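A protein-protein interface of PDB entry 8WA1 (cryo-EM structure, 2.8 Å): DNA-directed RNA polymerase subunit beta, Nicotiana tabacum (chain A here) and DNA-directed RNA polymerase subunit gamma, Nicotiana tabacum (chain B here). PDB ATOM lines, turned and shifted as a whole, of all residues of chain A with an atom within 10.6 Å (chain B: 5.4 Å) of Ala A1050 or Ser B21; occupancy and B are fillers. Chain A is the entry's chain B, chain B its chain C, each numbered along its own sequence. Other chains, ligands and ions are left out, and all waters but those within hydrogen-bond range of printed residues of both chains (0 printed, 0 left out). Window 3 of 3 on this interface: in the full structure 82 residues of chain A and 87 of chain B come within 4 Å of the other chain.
N of Glu A1052 is in hydrogen-bond range of O of Gly B20 (3.2 Å).
The backbone carbonyl oxygen of Leu A1046 sits at hydrogen-bond distance from the backbone NH of Leu A1051, at 2.6 Å.
The side-chain hydroxyl of Ser B21 is in hydrogen-bond range of the side-chain hydroxyl of Tyr B125 (2.9 Å).
Among the printed residues, pairs that only touch across the chains: Glu A1052 with Ile B19 (3.2 Å), Ala A1050 with Val B22 (3.3 Å), Arg A1047 with Trp B30 (3.4 Å), Glu A1052 with Val B22 (3.5 Å), Glu A1052 with Trp B30 (3.5 Å), Arg A1047 with Pro B277 (3.6 Å), Leu A1051 with Gly B20 (3.6 Å), Leu A1049 with His B122 (3.8 Å), Ala A1050 with Gly B20 (3.9 Å), Ala A1050 with Ser B21 (3.9 Å) and Leu A1051 with Val B22 (3.97 Å).
Ala A1050 touches just these residues of chain B: Gly B20, Ser B21 and Val B22.
Ser B21 touches just one residue of chain A: Ala A1050.
Val B22 touches three residues of chain A.
No residue of chain A comes within 4 Å of Ser B23.
No residue of chain A comes within 4 Å of Trp B270.
Printed residues of chain B within 4 Å of Leu A1049: His B122.
Of the printed residues of chain A, Trp B30 touches Arg A1047 (3.4 Å) and Glu A1052 (3.5 Å).
Printed residues of chain B within 4 Å of Arg A1047: Trp B30 (3.4 Å) and Pro B277 (3.6 Å).
Printed residues of chain B within 4 Å of Glu A1052: Ile B19 (3.2 Å), Gly B20 (3.2 Å), Val B22 (3.5 Å) and Trp B30 (3.5 Å).
Leu B273 touches none of the printed residues of chain A.
Glu A1045 touches none of the printed residues of chain B.
The nearest residue of chain B that does not touch Ala A1050 is Leu B273 (4.3 Å).
The nearest residue of chain A that does not touch Ser B21 is Leu A1051 (5.0 Å).
The nearest printed residue of chain A that does not touch Trp B30 is Leu A1051 (5.0 Å).
Along chain A the printed residues that touch a printed residue of chain B span positions 1047 to 1052.
Printed residues of chain B that touch a printed residue of chain A: Ile B19, Gly B20, Ser B21, Val B22, Trp B30, His B122 and Pro B277.
Hydrophobic or aromatic side chains of chain B that line the printed part of chain A: Ile B19, Val B22, Trp B30, His B122 and Pro B277.
Along chain B the printed residues that touch a printed residue of chain A span positions 19 to 277.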
ATOM      1  N   LEU A1042      -4.605  13.325  17.968  1.00  0.00           N
ATOM      2  CA  LEU A1042      -5.765  13.737  17.224  1.00  0.00           C
ATOM      3  C   LEU A1042      -6.505  14.741  18.031  1.00  0.00           C
ATOM      4  O   LEU A1042      -6.960  15.736  17.508  1.00  0.00           O
ATOM      5  CB  LEU A1042      -6.672  12.559  16.962  1.00  0.00           C
ATOM      6  CG  LEU A1042      -7.916  12.828  16.129  1.00  0.00           C
ATOM      7  CD1 LEU A1042      -7.513  13.235  14.724  1.00  0.00           C
ATOM      8  CD2 LEU A1042      -8.797  11.594  16.103  1.00  0.00           C
ATOM      9  N   VAL A1043      -6.619  14.504  19.322  1.00  0.00           N
ATOM     10  CA  VAL A1043      -7.404  15.402  20.112  1.00  0.00           C
ATOM     11  C   VAL A1043      -6.763  16.750  20.049  1.00  0.00           C
ATOM     12  O   VAL A1043      -7.437  17.739  19.828  1.00  0.00           O
ATOM     13  CB  VAL A1043      -7.463  14.955  21.555  1.00  0.00           C
ATOM     14  CG1 VAL A1043      -8.144  16.003  22.414  1.00  0.00           C
ATOM     15  CG2 VAL A1043      -8.206  13.640  21.656  1.00  0.00           C
ATOM     16  N   ARG A1044      -5.446  16.795  20.168  1.00  0.00           N
ATOM     17  CA  ARG A1044      -4.742  18.063  20.156  1.00  0.00           C
ATOM     18  C   ARG A1044      -4.905  18.763  18.833  1.00  0.00           C
ATOM     19  O   ARG A1044      -4.998  19.971  18.767  1.00  0.00           O
ATOM     20  CB  ARG A1044      -3.279  17.895  20.481  1.00  0.00           C
ATOM     21  CG  ARG A1044      -2.998  17.394  21.879  1.00  0.00           C
ATOM     22  CD  ARG A1044      -3.694  18.249  22.916  1.00  0.00           C
ATOM     23  NE  ARG A1044      -3.340  17.846  24.269  1.00  0.00           N
ATOM     24  CZ  ARG A1044      -3.958  16.887  24.945  1.00  0.00           C
ATOM     25  NH1 ARG A1044      -4.963  16.225  24.396  1.00  0.00           N
ATOM     26  NH2 ARG A1044      -3.567  16.586  26.173  1.00  0.00           N
ATOM     27  N   GLU A1045      -4.900  18.006  17.761  1.00  0.00           N
ATOM     28  CA  GLU A1045      -5.035  18.602  16.465  1.00  0.00           C
ATOM     29  C   GLU A1045      -6.425  19.144  16.307  1.00  0.00           C
ATOM     30  O   GLU A1045      -6.603  20.286  15.943  1.00  0.00           O
ATOM     31  CB  GLU A1045      -4.765  17.566  15.394  1.00  0.00           C
ATOM     32  CG  GLU A1045      -4.076  18.095  14.152  1.00  0.00           C
ATOM     33  CD  GLU A1045      -5.048  18.533  13.074  1.00  0.00           C
ATOM     34  OE1 GLU A1045      -6.269  18.528  13.324  1.00  0.00           O
ATOM     35  OE2 GLU A1045      -4.587  18.876  11.969  1.00  0.00           O
ATOM     36  N   LEU A1046      -7.420  18.317  16.553  1.00  0.00           N
ATOM     37  CA  LEU A1046      -8.808  18.745  16.422  1.00  0.00           C
ATOM     38  C   LEU A1046      -9.111  19.942  17.315  1.00  0.00           C
ATOM     39  O   LEU A1046      -9.892  20.821  16.936  1.00  0.00           O
ATOM     40  CB  LEU A1046      -9.753  17.586  16.739  1.00  0.00           C
ATOM     41  CG  LEU A1046      -9.781  16.446  15.721  1.00  0.00           C
ATOM     42  CD1 LEU A1046     -10.911  15.479  16.028  1.00  0.00           C
ATOM     43  CD2 LEU A1046      -9.906  16.989  14.306  1.00  0.00           C
ATOM     44  N   ARG A1047      -8.510  19.996  18.507  1.00  0.00           N
ATOM     45  CA  ARG A1047      -8.732  21.153  19.367  1.00  0.00           C
ATOM     46  C   ARG A1047      -7.954  22.371  18.890  1.00  0.00           C
ATOM     47  O   ARG A1047      -8.357  23.502  19.182  1.00  0.00           O
ATOM     48  CB  ARG A1047      -8.383  20.823  20.821  1.00  0.00           C
ATOM     49  CG  ARG A1047      -6.914  20.596  21.104  1.00  0.00           C
ATOM     50  CD  ARG A1047      -6.659  20.515  22.601  1.00  0.00           C
ATOM     51  NE  ARG A1047      -7.503  19.518  23.252  1.00  0.00           N
ATOM     52  CZ  ARG A1047      -7.500  19.275  24.559  1.00  0.00           C
ATOM     53  NH1 ARG A1047      -8.302  18.348  25.065  1.00  0.00           N
ATOM     54  NH2 ARG A1047      -6.694  19.958  25.360  1.00  0.00           N
ATOM     55  N   SER A1048      -6.851  22.168  18.165  1.00  0.00           N
ATOM     56  CA  SER A1048      -6.259  23.268  17.414  1.00  0.00           C
ATOM     57  C   SER A1048      -7.204  23.731  16.314  1.00  0.00           C
ATOM     58  O   SER A1048      -7.236  24.917  15.968  1.00  0.00           O
ATOM     59  CB  SER A1048      -4.913  22.843  16.829  1.00  0.00           C
ATOM     60  OG  SER A1048      -4.368  23.869  16.017  1.00  0.00           O
ATOM     61  N   LEU A1049      -7.981  22.805  15.755  1.00  0.00           N
ATOM     62  CA  LEU A1049      -9.055  23.131  14.829  1.00  0.00           C
ATOM     63  C   LEU A1049     -10.348  23.508  15.538  1.00  0.00           C
ATOM     64  O   LEU A1049     -11.409  23.516  14.902  1.00  0.00           O
ATOM     65  CB  LEU A1049      -9.317  21.956  13.886  1.00  0.00           C
ATOM     66  CG  LEU A1049      -8.381  21.822  12.690  1.00  0.00           C
ATOM     67  CD1 LEU A1049      -8.795  20.648  11.817  1.00  0.00           C
ATOM     68  CD2 LEU A1049      -8.384  23.117  11.896  1.00  0.00           C
ATOM     69  N   ALA A1050     -10.287  23.793  16.841  1.00  0.00           N
ATOM     70  CA  ALA A1050     -11.433  24.241  17.627  1.00  0.00           C
ATOM     71  C   ALA A1050     -12.515  23.171  17.723  1.00  0.00           C
ATOM     72  O   ALA A1050     -13.708  23.490  17.773  1.00  0.00           O
ATOM     73  CB  ALA A1050     -12.016  25.536  17.046  1.00  0.00           C
ATOM     74  N   LEU A1051     -12.113  21.901  17.743  1.00  0.00           N
ATOM     75  CA  LEU A1051     -13.038  20.779  17.877  1.00  0.00           C
ATOM     76  C   LEU A1051     -12.650  19.961  19.102  1.00  0.00           C
ATOM     77  O   LEU A1051     -11.485  19.574  19.252  1.00  0.00           O
ATOM     78  CB  LEU A1051     -13.022  19.902  16.624  1.00  0.00           C
ATOM     79  CG  LEU A1051     -13.206  20.622  15.286  1.00  0.00           C
ATOM     80  CD1 LEU A1051     -13.267  19.623  14.140  1.00  0.00           C
ATOM     81  CD2 LEU A1051     -14.452  21.493  15.312  1.00  0.00           C
ATOM     82  N   GLU A1052     -13.622  19.694  19.973  1.00  0.00           N
ATOM     83  CA  GLU A1052     -13.346  18.951  21.194  1.00  0.00           C
ATOM     84  C   GLU A1052     -13.538  17.450  20.982  1.00  0.00           C
ATOM     85  O   GLU A1052     -14.213  17.003  20.051  1.00  0.00           O
ATOM     86  CB  GLU A1052     -14.245  19.431  22.333  1.00  0.00           C
ATOM     87  CG  GLU A1052     -13.535  20.294  23.361  1.00  0.00           C
ATOM     88  CD  GLU A1052     -14.404  20.598  24.564  1.00  0.00           C
ATOM     89  OE1 GLU A1052     -15.616  20.294  24.514  1.00  0.00           O
ATOM     90  OE2 GLU A1052     -13.878  21.136  25.560  1.00  0.00           O
ATOM     91  N   LEU A1053     -12.930  16.671  21.875  1.00  0.00           N
ATOM     92  CA  LEU A1053     -13.071  15.216  21.871  1.00  0.00           C
ATOM     93  C   LEU A1053     -12.775  14.713  23.275  1.00  0.00           C
ATOM     94  O   LEU A1053     -11.671  14.920  23.787  1.00  0.00           O
ATOM     95  CB  LEU A1053     -12.138  14.566  20.850  1.00  0.00           C
ATOM     96  CG  LEU A1053     -12.751  14.162  19.508  1.00  0.00           C
ATOM     97  CD1 LEU A1053     -11.799  13.262  18.734  1.00  0.00           C
ATOM     98  CD2 LEU A1053     -14.095  13.480  19.714  1.00  0.00           C
ATOM     99  N   ASN A1054     -13.753  14.058  23.892  1.00  0.00           N
ATOM    100  CA  ASN A1054     -13.603  13.514  25.236  1.00  0.00           C
ATOM    101  C   ASN A1054     -14.085  12.073  25.248  1.00  0.00           C
ATOM    102  O   ASN A1054     -15.083  11.743  24.599  1.00  0.00           O
ATOM    103  CB  ASN A1054     -14.380  14.351  26.258  1.00  0.00           C
ATOM    104  CG  ASN A1054     -13.913  15.794  26.306  1.00  0.00           C
ATOM    105  OD1 ASN A1054     -12.725  16.079  26.159  1.00  0.00           O
ATOM    106  ND2 ASN A1054     -14.850  16.714  26.509  1.00  0.00           N
ATOM    107  N   ILE B  19     -18.127  15.364  20.368  1.00  0.00           N
ATOM    108  CA  ILE B  19     -17.456  16.384  19.578  1.00  0.00           C
ATOM    109  C   ILE B  19     -18.376  17.595  19.477  1.00  0.00           C
ATOM    110  O   ILE B  19     -19.601  17.477  19.487  1.00  0.00           O
ATOM    111  CB  ILE B  19     -17.063  15.869  18.175  1.00  0.00           C
ATOM    112  CG1 ILE B  19     -16.130  16.858  17.471  1.00  0.00           C
ATOM    113  CG2 ILE B  19     -18.302  15.610  17.333  1.00  0.00           C
ATOM    114  CD1 ILE B  19     -15.670  16.397  16.108  1.00  0.00           C
ATOM    115  N   GLY B  20     -17.766  18.771  19.391  1.00  0.00           N
ATOM    116  CA  GLY B  20     -18.532  19.998  19.283  1.00  0.00           C
ATOM    117  C   GLY B  20     -17.609  21.188  19.150  1.00  0.00           C
ATOM    118  O   GLY B  20     -16.381  21.069  19.247  1.00  0.00           O
ATOM    119  N   SER B  21     -18.222  22.344  18.922  1.00  0.00           N
ATOM    120  CA  SER B  21     -17.510  23.609  18.834  1.00  0.00           C
ATOM    121  C   SER B  21     -17.215  24.110  20.238  1.00  0.00           C
ATOM    122  O   SER B  21     -18.073  24.043  21.126  1.00  0.00           O
ATOM    123  CB  SER B  21     -18.318  24.653  18.060  1.00  0.00           C
ATOM    124  OG  SER B  21     -18.327  24.363  16.673  1.00  0.00           O
ATOM    125  N   VAL B  22     -16.001  24.609  20.437  1.00  0.00           N
ATOM    126  CA  VAL B  22     -15.530  25.011  21.753  1.00  0.00           C
ATOM    127  C   VAL B  22     -15.578  26.528  21.858  1.00  0.00           C
ATOM    128  O   VAL B  22     -15.300  27.251  20.896  1.00  0.00           O
ATOM    129  CB  VAL B  22     -14.108  24.482  22.032  1.00  0.00           C
ATOM    130  CG1 VAL B  22     -14.017  23.955  23.447  1.00  0.00           C
ATOM    131  CG2 VAL B  22     -13.738  23.394  21.038  1.00  0.00           C
ATOM    132  N   SER B  23     -15.942  27.006  23.044  1.00  0.00           N
ATOM    133  CA  SER B  23     -15.982  28.433  23.299  1.00  0.00           C
ATOM    134  C   SER B  23     -14.564  28.981  23.440  1.00  0.00           C
ATOM    135  O   SER B  23     -13.622  28.228  23.698  1.00  0.00           O
ATOM    136  CB  SER B  23     -16.788  28.719  24.564  1.00  0.00           C
ATOM    137  OG  SER B  23     -16.183  28.127  25.699  1.00  0.00           O
ATOM    138  N   TRP B  30      -7.431  25.963  28.156  1.00  0.00           N
ATOM    139  CA  TRP B  30      -6.498  24.936  27.712  1.00  0.00           C
ATOM    140  C   TRP B  30      -5.049  25.390  27.794  1.00  0.00           C
ATOM    141  O   TRP B  30      -4.150  24.543  27.820  1.00  0.00           O
ATOM    142  CB  TRP B  30      -6.796  24.519  26.269  1.00  0.00           C
ATOM    143  CG  TRP B  30      -8.080  23.785  26.087  1.00  0.00           C
ATOM    144  CD1 TRP B  30      -8.821  23.174  27.053  1.00  0.00           C
ATOM    145  CD2 TRP B  30      -8.781  23.589  24.857  1.00  0.00           C
ATOM    146  NE1 TRP B  30      -9.942  22.605  26.498  1.00  0.00           N
ATOM    147  CE2 TRP B  30      -9.940  22.847  25.150  1.00  0.00           C
ATOM    148  CE3 TRP B  30      -8.540  23.968  23.532  1.00  0.00           C
ATOM    149  CZ2 TRP B  30     -10.857  22.478  24.170  1.00  0.00           C
ATOM    150  CZ3 TRP B  30      -9.451  23.602  22.562  1.00  0.00           C
ATOM    151  CH2 TRP B  30     -10.595  22.863  22.885  1.00  0.00           C
ATOM    152  N   HIS B 122     -14.626  30.900  10.596  1.00  0.00           N
ATOM    153  CA  HIS B 122     -14.155  29.560  10.280  1.00  0.00           C
ATOM    154  C   HIS B 122     -14.405  29.250   8.809  1.00  0.00           C
ATOM    155  O   HIS B 122     -15.493  29.506   8.284  1.00  0.00           O
ATOM    156  CB  HIS B 122     -14.849  28.531  11.170  1.00  0.00           C
ATOM    157  CG  HIS B 122     -14.059  27.277  11.372  1.00  0.00           C
ATOM    158  ND1 HIS B 122     -13.969  26.291  10.414  1.00  0.00           N
ATOM    159  CD2 HIS B 122     -13.322  26.848  12.425  1.00  0.00           C
ATOM    160  CE1 HIS B 122     -13.211  25.309  10.866  1.00  0.00           C
ATOM    161  NE2 HIS B 122     -12.805  25.621  12.084  1.00  0.00           N
ATOM    162  N   TYR B 125     -17.275  26.463   8.059  1.00  0.00           N
ATOM    163  CA  TYR B 125     -18.673  26.874   8.133  1.00  0.00           C
ATOM    164  C   TYR B 125     -19.027  27.832   7.001  1.00  0.00           C
ATOM    165  O   TYR B 125     -20.133  27.776   6.450  1.00  0.00           O
ATOM    166  CB  TYR B 125     -18.954  27.514   9.491  1.00  0.00           C
ATOM    167  CG  TYR B 125     -18.676  26.597  10.659  1.00  0.00           C
ATOM    168  CD1 TYR B 125     -18.941  25.237  10.576  1.00  0.00           C
ATOM    169  CD2 TYR B 125     -18.139  27.089  11.841  1.00  0.00           C
ATOM    170  CE1 TYR B 125     -18.687  24.393  11.639  1.00  0.00           C
ATOM    171  CE2 TYR B 125     -17.882  26.253  12.909  1.00  0.00           C
ATOM    172  CZ  TYR B 125     -18.157  24.907  12.803  1.00  0.00           C
ATOM    173  OH  TYR B 125     -17.900  24.074  13.867  1.00  0.00           O
ATOM    174  N   ILE B 266     -24.591  24.165  22.554  1.00  0.00           N
ATOM    175  CA  ILE B 266     -23.596  24.771  21.681  1.00  0.00           C
ATOM    176  C   ILE B 266     -24.207  26.030  21.082  1.00  0.00           C
ATOM    177  O   ILE B 266     -25.372  26.043  20.673  1.00  0.00           O
ATOM    178  CB  ILE B 266     -23.124  23.804  20.567  1.00  0.00           C
ATOM    179  CG1 ILE B 266     -22.520  22.535  21.173  1.00  0.00           C
ATOM    180  CG2 ILE B 266     -22.116  24.479  19.653  1.00  0.00           C
ATOM    181  CD1 ILE B 266     -21.261  22.774  21.973  1.00  0.00           C
ATOM    182  N   TRP B 270     -19.954  30.685  18.495  1.00  0.00           N
ATOM    183  CA  TRP B 270     -18.624  30.090  18.460  1.00  0.00           C
ATOM    184  C   TRP B 270     -18.151  29.762  17.050  1.00  0.00           C
ATOM    185  O   TRP B 270     -17.016  29.298  16.895  1.00  0.00           O
ATOM    186  CB  TRP B 270     -18.604  28.833  19.331  1.00  0.00           C
ATOM    187  CG  TRP B 270     -19.040  29.086  20.746  1.00  0.00           C
ATOM    188  CD1 TRP B 270     -19.070  30.288  21.392  1.00  0.00           C
ATOM    189  CD2 TRP B 270     -19.520  28.116  21.685  1.00  0.00           C
ATOM    190  NE1 TRP B 270     -19.533  30.126  22.675  1.00  0.00           N
ATOM    191  CE2 TRP B 270     -19.816  28.802  22.880  1.00  0.00           C
ATOM    192  CE3 TRP B 270     -19.725  26.734  21.631  1.00  0.00           C
ATOM    193  CZ2 TRP B 270     -20.306  28.153  24.010  1.00  0.00           C
ATOM    194  CZ3 TRP B 270     -20.210  26.091  22.757  1.00  0.00           C
ATOM    195  CH2 TRP B 270     -20.496  26.801  23.929  1.00  0.00           C
ATOM    196  N   LEU B 273     -14.370  32.839  15.284  1.00  0.00           N
ATOM    197  CA  LEU B 273     -13.336  32.575  16.281  1.00  0.00           C
ATOM    198  C   LEU B 273     -12.784  33.896  16.803  1.00  0.00           C
ATOM    199  O   LEU B 273     -12.162  34.657  16.056  1.00  0.00           O
ATOM    200  CB  LEU B 273     -12.216  31.720  15.693  1.00  0.00           C
ATOM    201  CG  LEU B 273     -12.577  30.378  15.051  1.00  0.00           C
ATOM    202  CD1 LEU B 273     -12.862  30.545  13.566  1.00  0.00           C
ATOM    203  CD2 LEU B 273     -11.467  29.365  15.277  1.00  0.00           C
ATOM    204  N   PRO B 277      -6.549  28.778  18.858  1.00  0.00           N
ATOM    205  CA  PRO B 277      -5.625  27.921  19.611  1.00  0.00           C
ATOM    206  C   PRO B 277      -4.343  27.660  18.831  1.00  0.00           C
ATOM    207  O   PRO B 277      -4.302  27.779  17.605  1.00  0.00           O
ATOM    208  CB  PRO B 277      -6.427  26.629  19.821  1.00  0.00           C
ATOM    209  CG  PRO B 277      -7.856  27.017  19.596  1.00  0.00           C
ATOM    210  CD  PRO B 277      -7.815  28.092  18.560  1.00  0.00           C
